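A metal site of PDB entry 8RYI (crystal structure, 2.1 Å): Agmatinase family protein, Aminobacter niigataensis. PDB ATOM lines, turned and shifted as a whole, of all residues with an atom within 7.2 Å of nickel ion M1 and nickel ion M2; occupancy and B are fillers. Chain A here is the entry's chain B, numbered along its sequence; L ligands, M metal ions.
A ring nitrogen (NE2) of His 200 sits close to the side-chain carboxylate (OD2) of Asp 202. The backbone NH (N) of His 177 lies within hydrogen-bond range of the side-chain carboxylate (OE2) of Glu 339, at 2.7 Å. The side-chain carboxylate (OD2) of Asp 206 sits close to a ring nitrogen (NE2) of His 200 (3.4 Å). The side-chain carboxylate (OD1) of Asp 297 sits close to the backbone NH (N) of Cys 203. The backbone carbonyl oxygen of Asp 295 sits at hydrogen-bond distance from the side-chain hydroxyl of Ser 298, at 2.9 Å. The backbone carbonyl oxygen of Val 201 sits at hydrogen-bond distance from the backbone NH of Asp 295, 2.8 Å away. The side-chain carboxylate (OE2) of Glu 311 lies within hydrogen-bond range of a ring nitrogen (NE2) of His 204, 2.6 Å away. A ring nitrogen (NE2) of His 238 lies within hydrogen-bond range of the backbone carbonyl oxygen of His 204.
Within 4 Å of nickel ion M1: His 177, Asp 202, Asp 206 and Asp 295.
Within 4 Å of nickel ion M2: Asp 202, His 204, Asp 295 and Asp 297. The nearest printed residue that does not touch nickel ion M2 is Cys 203 (4.4 Å).
Nickel ion M1 is bound by OD2 of Asp 202 (2.1 Å), ND1 of His 177 (2.1 Å), OD2 of Asp 206 (2.2 Å), O1 of the ligand (2.2 Å) and OD2 of Asp 295 (2.5 Å).
Nickel ion M2 is bound by OD2 of Asp 297 (2.2 Å), O1 of the ligand (2.3 Å), OD1 of Asp 202 (2.3 Å), OD2 of Asp 295 (2.4 Å), ND1 of His 204 (2.4 Å) and OD1 of Asp 297 (2.5 Å). Nickel ion M2 has six donor atoms within binding distance. Slightly farther from nickel ion M2 lies a nitrogen (N2) of the ligand (2.8 Å).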
ATOM      1  N   ASP A 176      16.194 -33.973 -22.604  1.00  0.00           N
ATOM      2  CA  ASP A 176      15.047 -33.485 -23.362  1.00  0.00           C
ATOM      3  C   ASP A 176      14.264 -32.475 -22.512  1.00  0.00           C
ATOM      4  O   ASP A 176      14.545 -32.242 -21.326  1.00  0.00           O
ATOM      5  CB  ASP A 176      14.159 -34.643 -23.837  1.00  0.00           C
ATOM      6  CG  ASP A 176      13.548 -35.457 -22.692  1.00  0.00           C
ATOM      7  OD1 ASP A 176      13.049 -34.863 -21.697  1.00  0.00           O
ATOM      8  OD2 ASP A 176      13.546 -36.712 -22.781  1.00  0.00           O
ATOM      9  N   HIS A 177      13.240 -31.876 -23.137  1.00  0.00           N
ATOM     10  CA  HIS A 177      12.492 -30.818 -22.484  1.00  0.00           C
ATOM     11  C   HIS A 177      11.471 -31.318 -21.472  1.00  0.00           C
ATOM     12  O   HIS A 177      10.557 -30.551 -21.122  1.00  0.00           O
ATOM     13  CB  HIS A 177      11.799 -29.950 -23.527  1.00  0.00           C
ATOM     14  CG  HIS A 177      11.790 -28.500 -23.164  1.00  0.00           C
ATOM     15  ND1 HIS A 177      11.466 -27.495 -24.063  1.00  0.00           N
ATOM     16  CD2 HIS A 177      12.059 -27.885 -21.995  1.00  0.00           C
ATOM     17  CE1 HIS A 177      11.541 -26.331 -23.449  1.00  0.00           C
ATOM     18  NE2 HIS A 177      11.902 -26.543 -22.195  1.00  0.00           N
ATOM     19  N   SER A 178      11.551 -32.574 -21.022  1.00  0.00           N
ATOM     20  CA  SER A 178      10.814 -32.951 -19.829  1.00  0.00           C
ATOM     21  C   SER A 178      11.436 -32.343 -18.575  1.00  0.00           C
ATOM     22  O   SER A 178      10.783 -32.319 -17.521  1.00  0.00           O
ATOM     23  CB  SER A 178      10.738 -34.483 -19.708  1.00  0.00           C
ATOM     24  OG  SER A 178      11.992 -35.095 -19.389  1.00  0.00           O
ATOM     25  N   HIS A 200       9.232 -19.868 -20.573  1.00  0.00           N
ATOM     26  CA  HIS A 200       9.465 -21.003 -21.465  1.00  0.00           C
ATOM     27  C   HIS A 200       9.834 -20.419 -22.824  1.00  0.00           C
ATOM     28  O   HIS A 200       9.017 -19.741 -23.437  1.00  0.00           O
ATOM     29  CB  HIS A 200       8.203 -21.866 -21.531  1.00  0.00           C
ATOM     30  CG  HIS A 200       8.394 -23.190 -22.198  1.00  0.00           C
ATOM     31  ND1 HIS A 200       8.250 -24.387 -21.519  1.00  0.00           N
ATOM     32  CD2 HIS A 200       8.703 -23.516 -23.474  1.00  0.00           C
ATOM     33  CE1 HIS A 200       8.481 -25.387 -22.346  1.00  0.00           C
ATOM     34  NE2 HIS A 200       8.762 -24.895 -23.537  1.00  0.00           N
ATOM     35  N   VAL A 201      11.080 -20.619 -23.277  1.00  0.00           N
ATOM     36  CA  VAL A 201      11.559 -20.051 -24.544  1.00  0.00           C
ATOM     37  C   VAL A 201      11.851 -21.198 -25.517  1.00  0.00           C
ATOM     38  O   VAL A 201      12.660 -22.084 -25.225  1.00  0.00           O
ATOM     39  CB  VAL A 201      12.776 -19.152 -24.324  1.00  0.00           C
ATOM     40  CG1 VAL A 201      13.327 -18.700 -25.660  1.00  0.00           C
ATOM     41  CG2 VAL A 201      12.363 -17.911 -23.476  1.00  0.00           C
ATOM     42  N   ASP A 202      11.191 -21.179 -26.678  1.00  0.00           N
ATOM     43  CA  ASP A 202      11.068 -22.425 -27.423  1.00  0.00           C
ATOM     44  C   ASP A 202      10.491 -22.127 -28.794  1.00  0.00           C
ATOM     45  O   ASP A 202       9.677 -21.219 -28.947  1.00  0.00           O
ATOM     46  CB  ASP A 202      10.136 -23.390 -26.654  1.00  0.00           C
ATOM     47  CG  ASP A 202      10.333 -24.859 -27.012  1.00  0.00           C
ATOM     48  OD1 ASP A 202      10.552 -25.222 -28.174  1.00  0.00           O
ATOM     49  OD2 ASP A 202      10.231 -25.665 -26.089  1.00  0.00           O
ATOM     50  N   CYS A 203      10.890 -22.924 -29.785  1.00  0.00           N
ATOM     51  CA  CYS A 203      10.195 -22.848 -31.064  1.00  0.00           C
ATOM     52  C   CYS A 203       8.797 -23.429 -30.940  1.00  0.00           C
ATOM     53  O   CYS A 203       7.886 -23.093 -31.715  1.00  0.00           O
ATOM     54  CB  CYS A 203      10.954 -23.595 -32.163  1.00  0.00           C
ATOM     55  SG  CYS A 203      10.077 -23.570 -33.755  1.00  0.00           S
ATOM     56  N   HIS A 204       8.622 -24.321 -29.965  1.00  0.00           N
ATOM     57  CA  HIS A 204       7.411 -25.116 -29.809  1.00  0.00           C
ATOM     58  C   HIS A 204       6.694 -24.725 -28.530  1.00  0.00           C
ATOM     59  O   HIS A 204       7.324 -24.405 -27.523  1.00  0.00           O
ATOM     60  CB  HIS A 204       7.801 -26.604 -29.840  1.00  0.00           C
ATOM     61  CG  HIS A 204       8.632 -26.959 -31.038  1.00  0.00           C
ATOM     62  ND1 HIS A 204       9.972 -27.256 -30.958  1.00  0.00           N
ATOM     63  CD2 HIS A 204       8.315 -27.004 -32.353  1.00  0.00           C
ATOM     64  CE1 HIS A 204      10.441 -27.485 -32.171  1.00  0.00           C
ATOM     65  NE2 HIS A 204       9.459 -27.338 -33.034  1.00  0.00           N
ATOM     66  N   LEU A 205       5.351 -24.735 -28.595  1.00  0.00           N
ATOM     67  CA  LEU A 205       4.543 -24.258 -27.477  1.00  0.00           C
ATOM     68  C   LEU A 205       4.562 -25.219 -26.280  1.00  0.00           C
ATOM     69  O   LEU A 205       4.285 -24.794 -25.159  1.00  0.00           O
ATOM     70  CB  LEU A 205       3.103 -23.962 -27.968  1.00  0.00           C
ATOM     71  CG  LEU A 205       2.978 -22.783 -28.957  1.00  0.00           C
ATOM     72  CD1 LEU A 205       1.655 -22.739 -29.733  1.00  0.00           C
ATOM     73  CD2 LEU A 205       3.213 -21.450 -28.230  1.00  0.00           C
ATOM     74  N   ASP A 206       4.903 -26.512 -26.502  1.00  0.00           N
ATOM     75  CA  ASP A 206       5.070 -27.486 -25.408  1.00  0.00           C
ATOM     76  C   ASP A 206       3.944 -27.417 -24.370  1.00  0.00           C
ATOM     77  O   ASP A 206       4.176 -27.232 -23.171  1.00  0.00           O
ATOM     78  CB  ASP A 206       6.436 -27.287 -24.705  1.00  0.00           C
ATOM     79  CG  ASP A 206       7.614 -27.814 -25.529  1.00  0.00           C
ATOM     80  OD1 ASP A 206       7.491 -28.027 -26.749  1.00  0.00           O
ATOM     81  OD2 ASP A 206       8.698 -28.022 -24.928  1.00  0.00           O
ATOM     82  N   ASN A 218       8.176 -34.419 -22.879  1.00  0.00           N
ATOM     83  CA  ASN A 218       8.871 -33.171 -23.134  1.00  0.00           C
ATOM     84  C   ASN A 218       8.043 -32.174 -23.921  1.00  0.00           C
ATOM     85  O   ASN A 218       8.598 -31.174 -24.386  1.00  0.00           O
ATOM     86  CB  ASN A 218      10.203 -33.447 -23.855  1.00  0.00           C
ATOM     87  CG  ASN A 218      10.015 -33.972 -25.279  1.00  0.00           C
ATOM     88  OD1 ASN A 218       9.073 -34.703 -25.581  1.00  0.00           O
ATOM     89  ND2 ASN A 218      10.972 -33.617 -26.167  1.00  0.00           N
ATOM     90  N   CYS A 219       6.730 -32.391 -24.069  1.00  0.00           N
ATOM     91  CA  CYS A 219       5.884 -31.365 -24.660  1.00  0.00           C
ATOM     92  C   CYS A 219       4.858 -30.826 -23.658  1.00  0.00           C
ATOM     93  O   CYS A 219       3.829 -30.272 -24.064  1.00  0.00           O
ATOM     94  CB  CYS A 219       5.190 -31.884 -25.922  1.00  0.00           C
ATOM     95  SG  CYS A 219       3.830 -33.053 -25.616  1.00  0.00           S
ATOM     96  N   HIS A 238       5.489 -17.526 -22.727  1.00  0.00           N
ATOM     97  CA  HIS A 238       6.179 -18.332 -23.720  1.00  0.00           C
ATOM     98  C   HIS A 238       6.728 -17.402 -24.786  1.00  0.00           C
ATOM     99  O   HIS A 238       6.022 -16.478 -25.212  1.00  0.00           O
ATOM    100  CB  HIS A 238       5.252 -19.375 -24.343  1.00  0.00           C
ATOM    101  CG  HIS A 238       5.971 -20.399 -25.166  1.00  0.00           C
ATOM    102  ND1 HIS A 238       6.603 -20.089 -26.354  1.00  0.00           N
ATOM    103  CD2 HIS A 238       6.156 -21.728 -24.972  1.00  0.00           C
ATOM    104  CE1 HIS A 238       7.151 -21.187 -26.852  1.00  0.00           C
ATOM    105  NE2 HIS A 238       6.877 -22.194 -26.032  1.00  0.00           N
ATOM    106  N   LEU A 245       5.127 -27.373 -36.135  1.00  0.00           N
ATOM    107  CA  LEU A 245       5.248 -28.450 -35.147  1.00  0.00           C
ATOM    108  C   LEU A 245       4.669 -27.911 -33.841  1.00  0.00           C
ATOM    109  O   LEU A 245       5.347 -27.702 -32.824  1.00  0.00           O
ATOM    110  CB  LEU A 245       6.704 -28.920 -35.008  1.00  0.00           C
ATOM    111  CG  LEU A 245       6.976 -30.068 -34.005  1.00  0.00           C
ATOM    112  CD1 LEU A 245       6.113 -31.279 -34.296  1.00  0.00           C
ATOM    113  CD2 LEU A 245       8.466 -30.502 -33.893  1.00  0.00           C
ATOM    114  N   TRP A 250      -1.808 -27.251 -28.023  1.00  0.00           N
ATOM    115  CA  TRP A 250      -0.718 -26.494 -27.407  1.00  0.00           C
ATOM    116  C   TRP A 250      -0.997 -24.994 -27.436  1.00  0.00           C
ATOM    117  O   TRP A 250      -0.667 -24.282 -26.475  1.00  0.00           O
ATOM    118  CB  TRP A 250       0.605 -26.780 -28.111  1.00  0.00           C
ATOM    119  CG  TRP A 250       1.094 -28.225 -28.038  1.00  0.00           C
ATOM    120  CD1 TRP A 250       0.435 -29.295 -27.504  1.00  0.00           C
ATOM    121  CD2 TRP A 250       2.334 -28.734 -28.530  1.00  0.00           C
ATOM    122  NE1 TRP A 250       1.193 -30.445 -27.634  1.00  0.00           N
ATOM    123  CE2 TRP A 250       2.368 -30.119 -28.262  1.00  0.00           C
ATOM    124  CE3 TRP A 250       3.416 -28.150 -29.205  1.00  0.00           C
ATOM    125  CZ2 TRP A 250       3.439 -30.931 -28.630  1.00  0.00           C
ATOM    126  CZ3 TRP A 250       4.480 -28.949 -29.557  1.00  0.00           C
ATOM    127  CH2 TRP A 250       4.488 -30.331 -29.266  1.00  0.00           C
ATOM    128  N   THR A 293      13.109 -21.896 -18.550  1.00  0.00           N
ATOM    129  CA  THR A 293      13.493 -23.026 -19.386  1.00  0.00           C
ATOM    130  C   THR A 293      13.687 -22.551 -20.822  1.00  0.00           C
ATOM    131  O   THR A 293      12.856 -21.804 -21.364  1.00  0.00           O
ATOM    132  CB  THR A 293      12.482 -24.177 -19.319  1.00  0.00           C
ATOM    133  OG1 THR A 293      12.930 -25.248 -20.152  1.00  0.00           O
ATOM    134  CG2 THR A 293      11.081 -23.757 -19.792  1.00  0.00           C
ATOM    135  N   TRP A 294      14.806 -22.970 -21.430  1.00  0.00           N
ATOM    136  CA  TRP A 294      15.247 -22.465 -22.723  1.00  0.00           C
ATOM    137  C   TRP A 294      15.570 -23.630 -23.648  1.00  0.00           C
ATOM    138  O   TRP A 294      16.602 -24.312 -23.467  1.00  0.00           O
ATOM    139  CB  TRP A 294      16.444 -21.521 -22.549  1.00  0.00           C
ATOM    140  CG  TRP A 294      16.767 -20.656 -23.739  1.00  0.00           C
ATOM    141  CD1 TRP A 294      16.203 -20.727 -24.980  1.00  0.00           C
ATOM    142  CD2 TRP A 294      17.701 -19.571 -23.779  1.00  0.00           C
ATOM    143  NE1 TRP A 294      16.737 -19.762 -25.805  1.00  0.00           N
ATOM    144  CE2 TRP A 294      17.662 -19.035 -25.084  1.00  0.00           C
ATOM    145  CE3 TRP A 294      18.580 -19.016 -22.848  1.00  0.00           C
ATOM    146  CZ2 TRP A 294      18.487 -17.973 -25.490  1.00  0.00           C
ATOM    147  CZ3 TRP A 294      19.394 -17.924 -23.252  1.00  0.00           C
ATOM    148  CH2 TRP A 294      19.342 -17.437 -24.566  1.00  0.00           C
ATOM    149  N   ASP A 295      14.716 -23.865 -24.633  1.00  0.00           N
ATOM    150  CA  ASP A 295      14.962 -24.942 -25.599  1.00  0.00           C
ATOM    151  C   ASP A 295      15.895 -24.432 -26.693  1.00  0.00           C
ATOM    152  O   ASP A 295      15.671 -23.356 -27.271  1.00  0.00           O
ATOM    153  CB  ASP A 295      13.643 -25.417 -26.198  1.00  0.00           C
ATOM    154  CG  ASP A 295      13.781 -26.664 -27.050  1.00  0.00           C
ATOM    155  OD1 ASP A 295      14.861 -26.939 -27.653  1.00  0.00           O
ATOM    156  OD2 ASP A 295      12.777 -27.380 -27.108  1.00  0.00           O
ATOM    157  N   THR A 296      16.951 -25.199 -26.989  1.00  0.00           N
ATOM    158  CA  THR A 296      17.887 -24.729 -28.013  1.00  0.00           C
ATOM    159  C   THR A 296      17.230 -24.570 -29.377  1.00  0.00           C
ATOM    160  O   THR A 296      17.762 -23.843 -30.212  1.00  0.00           O
ATOM    161  CB  THR A 296      19.122 -25.651 -28.145  1.00  0.00           C
ATOM    162  OG1 THR A 296      18.707 -27.007 -28.310  1.00  0.00           O
ATOM    163  CG2 THR A 296      20.020 -25.518 -26.920  1.00  0.00           C
ATOM    164  N   ASP A 297      16.094 -25.219 -29.646  1.00  0.00           N
ATOM    165  CA  ASP A 297      15.535 -24.986 -30.979  1.00  0.00           C
ATOM    166  C   ASP A 297      14.785 -23.654 -31.121  1.00  0.00           C
ATOM    167  O   ASP A 297      14.305 -23.346 -32.218  1.00  0.00           O
ATOM    168  CB  ASP A 297      14.644 -26.146 -31.423  1.00  0.00           C
ATOM    169  CG  ASP A 297      13.458 -26.363 -30.535  1.00  0.00           C
ATOM    170  OD1 ASP A 297      12.887 -25.388 -29.957  1.00  0.00           O
ATOM    171  OD2 ASP A 297      13.083 -27.550 -30.425  1.00  0.00           O
ATOM    172  N   SER A 298      14.709 -22.861 -30.054  1.00  0.00           N
ATOM    173  CA  SER A 298      14.313 -21.475 -30.259  1.00  0.00           C
ATOM    174  C   SER A 298      15.325 -20.756 -31.139  1.00  0.00           C
ATOM    175  O   SER A 298      14.981 -19.765 -31.795  1.00  0.00           O
ATOM    176  CB  SER A 298      14.212 -20.763 -28.901  1.00  0.00           C
ATOM    177  OG  SER A 298      15.504 -20.647 -28.297  1.00  0.00           O
ATOM    178  N   ALA A 309      14.895 -31.350 -32.976  1.00  0.00           N
ATOM    179  CA  ALA A 309      13.870 -30.721 -33.816  1.00  0.00           C
ATOM    180  C   ALA A 309      14.329 -29.322 -34.195  1.00  0.00           C
ATOM    181  O   ALA A 309      13.766 -28.319 -33.736  1.00  0.00           O
ATOM    182  CB  ALA A 309      12.533 -30.686 -33.074  1.00  0.00           C
ATOM    183  N   GLU A 311      14.877 -25.826 -36.139  1.00  0.00           N
ATOM    184  CA  GLU A 311      13.852 -25.065 -36.849  1.00  0.00           C
ATOM    185  C   GLU A 311      14.423 -23.780 -37.435  1.00  0.00           C
ATOM    186  O   GLU A 311      15.198 -23.085 -36.782  1.00  0.00           O
ATOM    187  CB  GLU A 311      12.703 -24.701 -35.908  1.00  0.00           C
ATOM    188  CG  GLU A 311      11.940 -25.894 -35.317  1.00  0.00           C
ATOM    189  CD  GLU A 311      10.656 -26.145 -36.095  1.00  0.00           C
ATOM    190  OE1 GLU A 311      10.521 -25.568 -37.199  1.00  0.00           O
ATOM    191  OE2 GLU A 311       9.778 -26.878 -35.587  1.00  0.00           O
ATOM    192  N   VAL A 338      17.946 -27.148 -22.887  1.00  0.00           N
ATOM    193  CA  VAL A 338      17.630 -28.529 -23.234  1.00  0.00           C
ATOM    194  C   VAL A 338      17.773 -28.774 -24.736  1.00  0.00           C
ATOM    195  O   VAL A 338      17.875 -27.861 -25.552  1.00  0.00           O
ATOM    196  CB  VAL A 338      16.201 -28.907 -22.790  1.00  0.00           C
ATOM    197  CG1 VAL A 338      16.072 -28.795 -21.288  1.00  0.00           C
ATOM    198  CG2 VAL A 338      15.186 -27.962 -23.490  1.00  0.00           C
ATOM    199  N   GLU A 339      17.754 -30.065 -25.067  1.00  0.00           N
ATOM    200  CA  GLU A 339      17.630 -30.659 -26.399  1.00  0.00           C
ATOM    201  C   GLU A 339      18.870 -30.541 -27.274  1.00  0.00           C
ATOM    202  O   GLU A 339      18.788 -30.891 -28.453  1.00  0.00           O
ATOM    203  CB  GLU A 339      16.404 -30.105 -27.141  1.00  0.00           C
ATOM    204  CG  GLU A 339      15.078 -30.254 -26.333  1.00  0.00           C
ATOM    205  CD  GLU A 339      14.387 -31.624 -26.484  1.00  0.00           C
ATOM    206  OE1 GLU A 339      14.913 -32.502 -27.205  1.00  0.00           O
ATOM    207  OE2 GLU A 339      13.311 -31.854 -25.881  1.00  0.00           O
HETATM  208  C1  LIG L   1      10.123 -29.668 -28.462  1.00  0.00           C
HETATM  209  O1  LIG L   1       9.890 -28.516 -27.984  1.00  0.00           O
HETATM  210  N1  LIG L   1       9.155 -30.591 -28.572  1.00  0.00           N
HETATM  211  N2  LIG L   1      11.369 -30.022 -28.848  1.00  0.00           N
HETATM  212 NI    NI M   1      10.598 -27.758 -25.988  1.00  0.00          NI
HETATM  213 NI    NI M   2      11.394 -27.178 -29.019  1.00  0.00          NI
